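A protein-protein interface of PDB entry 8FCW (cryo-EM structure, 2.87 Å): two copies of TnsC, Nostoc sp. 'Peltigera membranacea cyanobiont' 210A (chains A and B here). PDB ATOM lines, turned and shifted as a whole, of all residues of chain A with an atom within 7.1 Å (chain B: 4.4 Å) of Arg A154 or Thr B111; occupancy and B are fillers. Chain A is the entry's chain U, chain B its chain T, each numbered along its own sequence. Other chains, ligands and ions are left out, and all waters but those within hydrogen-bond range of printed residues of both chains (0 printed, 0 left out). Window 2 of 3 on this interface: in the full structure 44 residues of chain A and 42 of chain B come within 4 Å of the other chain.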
ATOM      1  N   TYR A 110     -23.789   2.867  -4.519  1.00  0.00           N
ATOM      2  CA  TYR A 110     -24.218   1.817  -5.422  1.00  0.00           C
ATOM      3  C   TYR A 110     -25.102   0.828  -4.698  1.00  0.00           C
ATOM      4  O   TYR A 110     -26.112   0.392  -5.253  1.00  0.00           O
ATOM      5  CB  TYR A 110     -23.012   1.115  -6.034  1.00  0.00           C
ATOM      6  CG  TYR A 110     -22.254   1.949  -7.031  1.00  0.00           C
ATOM      7  CD1 TYR A 110     -22.909   2.877  -7.815  1.00  0.00           C
ATOM      8  CD2 TYR A 110     -20.889   1.795  -7.203  1.00  0.00           C
ATOM      9  CE1 TYR A 110     -22.223   3.654  -8.726  1.00  0.00           C
ATOM     10  CE2 TYR A 110     -20.194   2.575  -8.104  1.00  0.00           C
ATOM     11  CZ  TYR A 110     -20.870   3.499  -8.868  1.00  0.00           C
ATOM     12  OH  TYR A 110     -20.208   4.277  -9.784  1.00  0.00           O
ATOM     13  N   TYR A 128     -28.892 -10.702 -11.459  1.00  0.00           N
ATOM     14  CA  TYR A 128     -27.995  -9.653 -11.925  1.00  0.00           C
ATOM     15  C   TYR A 128     -26.579 -10.154 -12.019  1.00  0.00           C
ATOM     16  O   TYR A 128     -26.184 -11.097 -11.319  1.00  0.00           O
ATOM     17  CB  TYR A 128     -28.050  -8.449 -10.990  1.00  0.00           C
ATOM     18  CG  TYR A 128     -29.397  -8.206 -10.355  1.00  0.00           C
ATOM     19  CD1 TYR A 128     -30.470  -7.778 -11.118  1.00  0.00           C
ATOM     20  CD2 TYR A 128     -29.594  -8.405  -9.002  1.00  0.00           C
ATOM     21  CE1 TYR A 128     -31.706  -7.597 -10.558  1.00  0.00           C
ATOM     22  CE2 TYR A 128     -30.827  -8.187  -8.420  1.00  0.00           C
ATOM     23  CZ  TYR A 128     -31.884  -7.782  -9.203  1.00  0.00           C
ATOM     24  OH  TYR A 128     -33.130  -7.547  -8.642  1.00  0.00           O
ATOM     25  N   GLY A 129     -25.800  -9.538 -12.886  1.00  0.00           N
ATOM     26  CA  GLY A 129     -24.394  -9.873 -12.964  1.00  0.00           C
ATOM     27  C   GLY A 129     -23.703  -9.735 -11.629  1.00  0.00           C
ATOM     28  O   GLY A 129     -24.183  -9.084 -10.715  1.00  0.00           O
ATOM     29  N   VAL A 130     -22.545 -10.341 -11.539  1.00  0.00           N
ATOM     30  CA  VAL A 130     -21.803 -10.509 -10.296  1.00  0.00           C
ATOM     31  C   VAL A 130     -22.567 -11.397  -9.336  1.00  0.00           C
ATOM     32  O   VAL A 130     -23.767 -11.232  -9.113  1.00  0.00           O
ATOM     33  CB  VAL A 130     -21.430  -9.167  -9.631  1.00  0.00           C
ATOM     34  CG1 VAL A 130     -20.221  -9.382  -8.736  1.00  0.00           C
ATOM     35  CG2 VAL A 130     -21.083  -8.116 -10.676  1.00  0.00           C
ATOM     36  N   ARG A 131     -21.854 -12.374  -8.806  1.00  0.00           N
ATOM     37  CA  ARG A 131     -22.475 -13.450  -8.075  1.00  0.00           C
ATOM     38  C   ARG A 131     -22.733 -13.076  -6.623  1.00  0.00           C
ATOM     39  O   ARG A 131     -23.383 -13.830  -5.904  1.00  0.00           O
ATOM     40  CB  ARG A 131     -21.590 -14.691  -8.153  1.00  0.00           C
ATOM     41  CG  ARG A 131     -20.675 -14.744  -9.370  1.00  0.00           C
ATOM     42  CD  ARG A 131     -21.449 -14.729 -10.686  1.00  0.00           C
ATOM     43  NE  ARG A 131     -20.550 -14.598 -11.832  1.00  0.00           N
ATOM     44  CZ  ARG A 131     -20.809 -15.040 -13.071  1.00  0.00           C
ATOM     45  NH1 ARG A 131     -21.934 -15.686 -13.348  1.00  0.00           N
ATOM     46  NH2 ARG A 131     -19.926 -14.852 -14.038  1.00  0.00           N
ATOM     47  N   ILE A 133     -24.561 -10.636  -5.456  1.00  0.00           N
ATOM     48  CA  ILE A 133     -25.810  -9.920  -5.273  1.00  0.00           C
ATOM     49  C   ILE A 133     -26.945 -10.864  -5.596  1.00  0.00           C
ATOM     50  O   ILE A 133     -26.973 -11.465  -6.674  1.00  0.00           O
ATOM     51  CB  ILE A 133     -25.881  -8.668  -6.162  1.00  0.00           C
ATOM     52  CG1 ILE A 133     -24.689  -7.747  -5.881  1.00  0.00           C
ATOM     53  CG2 ILE A 133     -27.185  -7.917  -5.931  1.00  0.00           C
ATOM     54  CD1 ILE A 133     -24.254  -6.937  -7.074  1.00  0.00           C
ATOM     55  N   VAL A 148     -16.814  -5.976  -5.033  1.00  0.00           N
ATOM     56  CA  VAL A 148     -16.050  -4.766  -5.246  1.00  0.00           C
ATOM     57  C   VAL A 148     -16.926  -3.717  -5.908  1.00  0.00           C
ATOM     58  O   VAL A 148     -17.951  -4.023  -6.516  1.00  0.00           O
ATOM     59  CB  VAL A 148     -14.800  -5.046  -6.092  1.00  0.00           C
ATOM     60  CG1 VAL A 148     -15.156  -5.214  -7.563  1.00  0.00           C
ATOM     61  CG2 VAL A 148     -13.736  -3.974  -5.897  1.00  0.00           C
ATOM     62  N   ALA A 149     -16.540  -2.456  -5.766  1.00  0.00           N
ATOM     63  CA  ALA A 149     -17.366  -1.355  -6.222  1.00  0.00           C
ATOM     64  C   ALA A 149     -17.657  -1.386  -7.719  1.00  0.00           C
ATOM     65  O   ALA A 149     -18.805  -1.141  -8.106  1.00  0.00           O
ATOM     66  CB  ALA A 149     -16.748  -0.034  -5.801  1.00  0.00           C
ATOM     67  N   PRO A 150     -16.657  -1.661  -8.582  1.00  0.00           N
ATOM     68  CA  PRO A 150     -16.995  -1.743 -10.002  1.00  0.00           C
ATOM     69  C   PRO A 150     -18.008  -2.827 -10.324  1.00  0.00           C
ATOM     70  O   PRO A 150     -18.818  -2.657 -11.249  1.00  0.00           O
ATOM     71  CB  PRO A 150     -15.658  -2.047 -10.650  1.00  0.00           C
ATOM     72  CG  PRO A 150     -14.677  -1.381  -9.747  1.00  0.00           C
ATOM     73  CD  PRO A 150     -15.202  -1.666  -8.376  1.00  0.00           C
ATOM     74  N   ALA A 151     -17.997  -3.921  -9.583  1.00  0.00           N
ATOM     75  CA  ALA A 151     -18.990  -4.965  -9.806  1.00  0.00           C
ATOM     76  C   ALA A 151     -20.372  -4.468  -9.466  1.00  0.00           C
ATOM     77  O   ALA A 151     -21.328  -4.742 -10.183  1.00  0.00           O
ATOM     78  CB  ALA A 151     -18.657  -6.198  -8.993  1.00  0.00           C
ATOM     79  N   LEU A 152     -20.495  -3.731  -8.368  1.00  0.00           N
ATOM     80  CA  LEU A 152     -21.779  -3.155  -8.003  1.00  0.00           C
ATOM     81  C   LEU A 152     -22.224  -2.173  -9.065  1.00  0.00           C
ATOM     82  O   LEU A 152     -23.406  -2.041  -9.354  1.00  0.00           O
ATOM     83  CB  LEU A 152     -21.695  -2.484  -6.639  1.00  0.00           C
ATOM     84  CG  LEU A 152     -21.629  -3.414  -5.430  1.00  0.00           C
ATOM     85  CD1 LEU A 152     -21.154  -2.614  -4.217  1.00  0.00           C
ATOM     86  CD2 LEU A 152     -22.994  -4.061  -5.185  1.00  0.00           C
ATOM     87  N   ARG A 153     -21.282  -1.456  -9.647  1.00  0.00           N
ATOM     88  CA  ARG A 153     -21.603  -0.515 -10.699  1.00  0.00           C
ATOM     89  C   ARG A 153     -22.149  -1.233 -11.904  1.00  0.00           C
ATOM     90  O   ARG A 153     -23.116  -0.786 -12.510  1.00  0.00           O
ATOM     91  CB  ARG A 153     -20.382   0.312 -11.073  1.00  0.00           C
ATOM     92  CG  ARG A 153     -20.726   1.618 -11.752  1.00  0.00           C
ATOM     93  CD  ARG A 153     -19.514   2.184 -12.455  1.00  0.00           C
ATOM     94  NE  ARG A 153     -19.860   2.746 -13.753  1.00  0.00           N
ATOM     95  CZ  ARG A 153     -19.617   4.003 -14.102  1.00  0.00           C
ATOM     96  NH1 ARG A 153     -19.012   4.837 -13.258  1.00  0.00           N
ATOM     97  NH2 ARG A 153     -19.968   4.425 -15.304  1.00  0.00           N
ATOM     98  N   ARG A 154     -21.539  -2.348 -12.274  1.00  0.00           N
ATOM     99  CA  ARG A 154     -22.023  -3.121 -13.404  1.00  0.00           C
ATOM    100  C   ARG A 154     -23.413  -3.658 -13.129  1.00  0.00           C
ATOM    101  O   ARG A 154     -24.281  -3.633 -14.003  1.00  0.00           O
ATOM    102  CB  ARG A 154     -21.072  -4.258 -13.750  1.00  0.00           C
ATOM    103  CG  ARG A 154     -21.420  -4.937 -15.070  1.00  0.00           C
ATOM    104  CD  ARG A 154     -20.491  -6.072 -15.424  1.00  0.00           C
ATOM    105  NE  ARG A 154     -19.171  -5.836 -14.875  1.00  0.00           N
ATOM    106  CZ  ARG A 154     -18.518  -6.682 -14.088  1.00  0.00           C
ATOM    107  NH1 ARG A 154     -19.063  -7.841 -13.755  1.00  0.00           N
ATOM    108  NH2 ARG A 154     -17.313  -6.367 -13.638  1.00  0.00           N
ATOM    109  N   ALA A 155     -23.646  -4.127 -11.916  1.00  0.00           N
ATOM    110  CA  ALA A 155     -24.962  -4.660 -11.586  1.00  0.00           C
ATOM    111  C   ALA A 155     -26.004  -3.575 -11.625  1.00  0.00           C
ATOM    112  O   ALA A 155     -27.109  -3.780 -12.127  1.00  0.00           O
ATOM    113  CB  ALA A 155     -24.948  -5.321 -10.229  1.00  0.00           C
ATOM    114  N   LEU A 156     -25.663  -2.401 -11.107  1.00  0.00           N
ATOM    115  CA  LEU A 156     -26.592  -1.277 -11.116  1.00  0.00           C
ATOM    116  C   LEU A 156     -26.865  -0.840 -12.532  1.00  0.00           C
ATOM    117  O   LEU A 156     -27.978  -0.472 -12.860  1.00  0.00           O
ATOM    118  CB  LEU A 156     -26.043  -0.121 -10.292  1.00  0.00           C
ATOM    119  CG  LEU A 156     -26.769   1.208 -10.339  1.00  0.00           C
ATOM    120  CD1 LEU A 156     -28.200   1.063  -9.880  1.00  0.00           C
ATOM    121  CD2 LEU A 156     -26.084   2.221  -9.439  1.00  0.00           C
ATOM    122  N   GLU A 157     -25.856  -0.882 -13.385  1.00  0.00           N
ATOM    123  CA  GLU A 157     -26.018  -0.533 -14.782  1.00  0.00           C
ATOM    124  C   GLU A 157     -26.988  -1.476 -15.440  1.00  0.00           C
ATOM    125  O   GLU A 157     -27.864  -1.044 -16.174  1.00  0.00           O
ATOM    126  CB  GLU A 157     -24.678  -0.535 -15.514  1.00  0.00           C
ATOM    127  CG  GLU A 157     -23.797   0.665 -15.223  1.00  0.00           C
ATOM    128  CD  GLU A 157     -22.476   0.643 -15.975  1.00  0.00           C
ATOM    129  OE1 GLU A 157     -22.302  -0.230 -16.852  1.00  0.00           O
ATOM    130  OE2 GLU A 157     -21.605   1.497 -15.685  1.00  0.00           O
ATOM    131  N   ASN A 158     -26.855  -2.770 -15.177  1.00  0.00           N
ATOM    132  CA  ASN A 158     -27.759  -3.737 -15.782  1.00  0.00           C
ATOM    133  C   ASN A 158     -29.167  -3.511 -15.308  1.00  0.00           C
ATOM    134  O   ASN A 158     -30.112  -3.527 -16.108  1.00  0.00           O
ATOM    135  CB  ASN A 158     -27.323  -5.152 -15.467  1.00  0.00           C
ATOM    136  CG  ASN A 158     -26.234  -5.642 -16.385  1.00  0.00           C
ATOM    137  OD1 ASN A 158     -25.067  -5.580 -16.044  1.00  0.00           O
ATOM    138  ND2 ASN A 158     -26.616  -6.133 -17.555  1.00  0.00           N
ATOM    139  N   ALA A 159     -29.336  -3.278 -14.016  1.00  0.00           N
ATOM    140  CA  ALA A 159     -30.672  -3.098 -13.478  1.00  0.00           C
ATOM    141  C   ALA A 159     -31.305  -1.844 -14.038  1.00  0.00           C
ATOM    142  O   ALA A 159     -32.478  -1.836 -14.388  1.00  0.00           O
ATOM    143  CB  ALA A 159     -30.630  -3.051 -11.968  1.00  0.00           C
ATOM    144  N   LEU A 160     -30.547  -0.760 -14.114  1.00  0.00           N
ATOM    145  CA  LEU A 160     -31.065   0.490 -14.636  1.00  0.00           C
ATOM    146  C   LEU A 160     -31.407   0.327 -16.098  1.00  0.00           C
ATOM    147  O   LEU A 160     -32.380   0.892 -16.575  1.00  0.00           O
ATOM    148  CB  LEU A 160     -30.049   1.610 -14.437  1.00  0.00           C
ATOM    149  CG  LEU A 160     -30.151   2.414 -13.144  1.00  0.00           C
ATOM    150  CD1 LEU A 160     -28.894   3.216 -12.903  1.00  0.00           C
ATOM    151  CD2 LEU A 160     -31.310   3.364 -13.196  1.00  0.00           C
ATOM    152  N   ILE A 161     -30.608  -0.432 -16.834  1.00  0.00           N
ATOM    153  CA  ILE A 161     -30.832  -0.579 -18.265  1.00  0.00           C
ATOM    154  C   ILE A 161     -32.117  -1.329 -18.476  1.00  0.00           C
ATOM    155  O   ILE A 161     -32.923  -0.947 -19.330  1.00  0.00           O
ATOM    156  CB  ILE A 161     -29.640  -1.260 -18.955  1.00  0.00           C
ATOM    157  CG1 ILE A 161     -28.499  -0.244 -19.148  1.00  0.00           C
ATOM    158  CG2 ILE A 161     -30.044  -1.866 -20.282  1.00  0.00           C
ATOM    159  CD1 ILE A 161     -27.250  -0.847 -19.745  1.00  0.00           C
ATOM    160  N   LEU A 195     -22.041   6.770 -15.584  1.00  0.00           N
ATOM    161  CA  LEU A 195     -23.135   5.920 -15.143  1.00  0.00           C
ATOM    162  C   LEU A 195     -24.396   6.249 -15.867  1.00  0.00           C
ATOM    163  O   LEU A 195     -25.162   5.356 -16.184  1.00  0.00           O
ATOM    164  CB  LEU A 195     -23.357   6.054 -13.643  1.00  0.00           C
ATOM    165  CG  LEU A 195     -24.419   5.172 -13.011  1.00  0.00           C
ATOM    166  CD1 LEU A 195     -24.132   3.714 -13.262  1.00  0.00           C
ATOM    167  CD2 LEU A 195     -24.510   5.443 -11.522  1.00  0.00           C
ATOM    168  N   LYS B 107      -9.053  -3.571 -15.032  1.00  0.00           N
ATOM    169  CA  LYS B 107      -9.731  -4.859 -14.957  1.00  0.00           C
ATOM    170  C   LYS B 107     -11.141  -4.762 -15.505  1.00  0.00           C
ATOM    171  O   LYS B 107     -11.601  -5.618 -16.255  1.00  0.00           O
ATOM    172  CB  LYS B 107      -9.747  -5.365 -13.522  1.00  0.00           C
ATOM    173  CG  LYS B 107     -10.144  -6.823 -13.368  1.00  0.00           C
ATOM    174  CD  LYS B 107     -10.075  -7.248 -11.910  1.00  0.00           C
ATOM    175  CE  LYS B 107     -10.432  -8.713 -11.738  1.00  0.00           C
ATOM    176  NZ  LYS B 107     -11.705  -9.090 -12.416  1.00  0.00           N
ATOM    177  N   GLU B 108     -11.834  -3.700 -15.149  1.00  0.00           N
ATOM    178  CA  GLU B 108     -13.185  -3.498 -15.640  1.00  0.00           C
ATOM    179  C   GLU B 108     -13.176  -3.263 -17.129  1.00  0.00           C
ATOM    180  O   GLU B 108     -14.064  -3.716 -17.838  1.00  0.00           O
ATOM    181  CB  GLU B 108     -13.853  -2.333 -14.932  1.00  0.00           C
ATOM    182  CG  GLU B 108     -15.014  -2.727 -14.028  1.00  0.00           C
ATOM    183  CD  GLU B 108     -16.209  -3.121 -14.831  1.00  0.00           C
ATOM    184  OE1 GLU B 108     -16.819  -2.225 -15.480  1.00  0.00           O
ATOM    185  OE2 GLU B 108     -16.541  -4.327 -14.837  1.00  0.00           O
ATOM    186  N   TYR B 109     -12.178  -2.558 -17.630  1.00  0.00           N
ATOM    187  CA  TYR B 109     -12.105  -2.291 -19.057  1.00  0.00           C
ATOM    188  C   TYR B 109     -11.920  -3.583 -19.805  1.00  0.00           C
ATOM    189  O   TYR B 109     -12.561  -3.828 -20.816  1.00  0.00           O
ATOM    190  CB  TYR B 109     -10.984  -1.307 -19.360  1.00  0.00           C
ATOM    191  CG  TYR B 109     -10.635  -1.192 -20.813  1.00  0.00           C
ATOM    192  CD1 TYR B 109     -11.333  -0.336 -21.645  1.00  0.00           C
ATOM    193  CD2 TYR B 109      -9.607  -1.939 -21.357  1.00  0.00           C
ATOM    194  CE1 TYR B 109     -11.016  -0.230 -22.987  1.00  0.00           C
ATOM    195  CE2 TYR B 109      -9.287  -1.844 -22.698  1.00  0.00           C
ATOM    196  CZ  TYR B 109      -9.997  -0.989 -23.503  1.00  0.00           C
ATOM    197  OH  TYR B 109      -9.673  -0.894 -24.822  1.00  0.00           O
ATOM    198  N   TYR B 110     -11.047  -4.441 -19.311  1.00  0.00           N
ATOM    199  CA  TYR B 110     -10.782  -5.709 -19.962  1.00  0.00           C
ATOM    200  C   TYR B 110     -12.017  -6.573 -19.936  1.00  0.00           C
ATOM    201  O   TYR B 110     -12.358  -7.199 -20.935  1.00  0.00           O
ATOM    202  CB  TYR B 110      -9.613  -6.418 -19.302  1.00  0.00           C
ATOM    203  CG  TYR B 110      -8.275  -5.825 -19.624  1.00  0.00           C
ATOM    204  CD1 TYR B 110      -8.042  -5.227 -20.853  1.00  0.00           C
ATOM    205  CD2 TYR B 110      -7.239  -5.867 -18.705  1.00  0.00           C
ATOM    206  CE1 TYR B 110      -6.820  -4.665 -21.151  1.00  0.00           C
ATOM    207  CE2 TYR B 110      -6.008  -5.305 -18.997  1.00  0.00           C
ATOM    208  CZ  TYR B 110      -5.813  -4.712 -20.220  1.00  0.00           C
ATOM    209  OH  TYR B 110      -4.606  -4.172 -20.515  1.00  0.00           O
ATOM    210  N   THR B 111     -12.708  -6.616 -18.808  1.00  0.00           N
ATOM    211  CA  THR B 111     -13.825  -7.539 -18.701  1.00  0.00           C
ATOM    212  C   THR B 111     -14.984  -7.045 -19.540  1.00  0.00           C
ATOM    213  O   THR B 111     -15.699  -7.832 -20.165  1.00  0.00           O
ATOM    214  CB  THR B 111     -14.238  -7.784 -17.243  1.00  0.00           C
ATOM    215  OG1 THR B 111     -15.235  -8.814 -17.207  1.00  0.00           O
ATOM    216  CG2 THR B 111     -14.773  -6.525 -16.603  1.00  0.00           C
ATOM    217  N   ARG B 112     -15.155  -5.736 -19.608  1.00  0.00           N
ATOM    218  CA  ARG B 112     -16.220  -5.155 -20.402  1.00  0.00           C
ATOM    219  C   ARG B 112     -15.916  -5.305 -21.879  1.00  0.00           C
ATOM    220  O   ARG B 112     -16.820  -5.516 -22.682  1.00  0.00           O
ATOM    221  CB  ARG B 112     -16.427  -3.694 -20.019  1.00  0.00           C
ATOM    222  CG  ARG B 112     -17.855  -3.211 -20.023  1.00  0.00           C
ATOM    223  CD  ARG B 112     -17.968  -1.864 -19.292  1.00  0.00           C
ATOM    224  NE  ARG B 112     -18.193  -2.015 -17.865  1.00  0.00           N
ATOM    225  CZ  ARG B 112     -19.386  -2.197 -17.299  1.00  0.00           C
ATOM    226  NH1 ARG B 112     -20.488  -2.239 -18.028  1.00  0.00           N
ATOM    227  NH2 ARG B 112     -19.481  -2.335 -15.974  1.00  0.00           N
ATOM    228  N   ALA B 113     -14.650  -5.211 -22.257  1.00  0.00           N
ATOM    229  CA  ALA B 113     -14.280  -5.461 -23.642  1.00  0.00           C
ATOM    230  C   ALA B 113     -14.527  -6.894 -24.023  1.00  0.00           C
ATOM    231  O   ALA B 113     -14.947  -7.193 -25.135  1.00  0.00           O
ATOM    232  CB  ALA B 113     -12.830  -5.090 -23.882  1.00  0.00           C
ATOM    233  N   LEU B 114     -14.242  -7.809 -23.113  1.00  0.00           N
ATOM    234  CA  LEU B 114     -14.499  -9.217 -23.361  1.00  0.00           C
ATOM    235  C   LEU B 114     -15.987  -9.454 -23.504  1.00  0.00           C
ATOM    236  O   LEU B 114     -16.418 -10.226 -24.347  1.00  0.00           O
ATOM    237  CB  LEU B 114     -13.913 -10.076 -22.256  1.00  0.00           C
ATOM    238  CG  LEU B 114     -13.776 -11.574 -22.559  1.00  0.00           C
ATOM    239  CD1 LEU B 114     -13.250 -11.786 -23.983  1.00  0.00           C
ATOM    240  CD2 LEU B 114     -12.853 -12.235 -21.538  1.00  0.00           C
ATOM    241  N   ILE B 115     -16.794  -8.806 -22.683  1.00  0.00           N
ATOM    242  CA  ILE B 115     -18.238  -8.955 -22.768  1.00  0.00           C
ATOM    243  C   ILE B 115     -18.751  -8.412 -24.100  1.00  0.00           C
ATOM    244  O   ILE B 115     -19.507  -9.075 -24.789  1.00  0.00           O
ATOM    245  CB  ILE B 115     -18.938  -8.270 -21.584  1.00  0.00           C
ATOM    246  CG1 ILE B 115     -18.590  -8.973 -20.268  1.00  0.00           C
ATOM    247  CG2 ILE B 115     -20.435  -8.224 -21.795  1.00  0.00           C
ATOM    248  CD1 ILE B 115     -19.441 -10.187 -19.959  1.00  0.00           C
ATOM    249  N   VAL B 143     -17.040 -13.833 -16.044  1.00  0.00           N
ATOM    250  CA  VAL B 143     -15.733 -13.435 -15.584  1.00  0.00           C
ATOM    251  C   VAL B 143     -15.798 -13.314 -14.083  1.00  0.00           C
ATOM    252  O   VAL B 143     -16.563 -12.499 -13.547  1.00  0.00           O
ATOM    253  CB  VAL B 143     -15.305 -12.104 -16.222  1.00  0.00           C
ATOM    254  CG1 VAL B 143     -14.121 -11.495 -15.482  1.00  0.00           C
ATOM    255  CG2 VAL B 143     -14.945 -12.314 -17.676  1.00  0.00           C
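OE1 of Glu B108 is in salt-bridge range of NH2 of Arg B112 (2.7 Å). The guanidinium group of Arg A153 is in salt-bridge range of the side-chain carboxylate of Glu A157 (2.9 Å). O of Arg A154 lies close to OD1 of Asn A158, at 2.9 Å.
The guanidinium group (NH2) of Arg A154 lies within salt-bridge range of the side-chain carboxylate (OE2) of Glu B108, at 2.5 Å. OE1 of Glu A157 is in salt-bridge range of NH1 of Arg B112 (3.0 Å).
1 position is printed for both chains.
Of the printed residues of chain B, Arg A154 touches Glu B108 (2.5 Å), Thr B111 (3.9 Å) and Arg B112 (3.3 Å). Thr B111 touches just one residue of chain A: Arg A154 (3.9 Å). Printed residues of chain B within 4 Å of Pro A150: Glu B108. Of the printed residues of chain A, Val B143 touches Arg A131 (3.7 Å). Of the printed residues of chain A, Glu B108 touches Pro A150 and Arg A154. Val A130 touches none of the printed residues of chain B. Leu B114 touches none of the printed residues of chain A. The nearest printed residue of chain B that does not touch Arg A154 is Val B143 (5.3 Å). The nearest printed residue of chain A that does not touch Thr B111 is Pro A150 (7.5 Å).
Val B143 touches Arg A131 (N to NH2, 3.7 Å). CB of Pro A150 touches CG of Glu B108, at 3.5 Å. Arg A154 touches Thr B111. CB of Arg A154 touches NH2 of Arg B112 (3.3 Å).
Of the 10 printed residues of chain B, 4 touch a printed residue of chain A. Among the printed residues, 6 pairs touch across the chains. Among the printed residues, Asp or Glu carboxylates within 4 Å of a Lys or Arg side-chain nitrogen of the other chain: Arg A154 with Glu B108 (2.5 Å) and Glu A157 with Arg B112 (3.0 Å).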
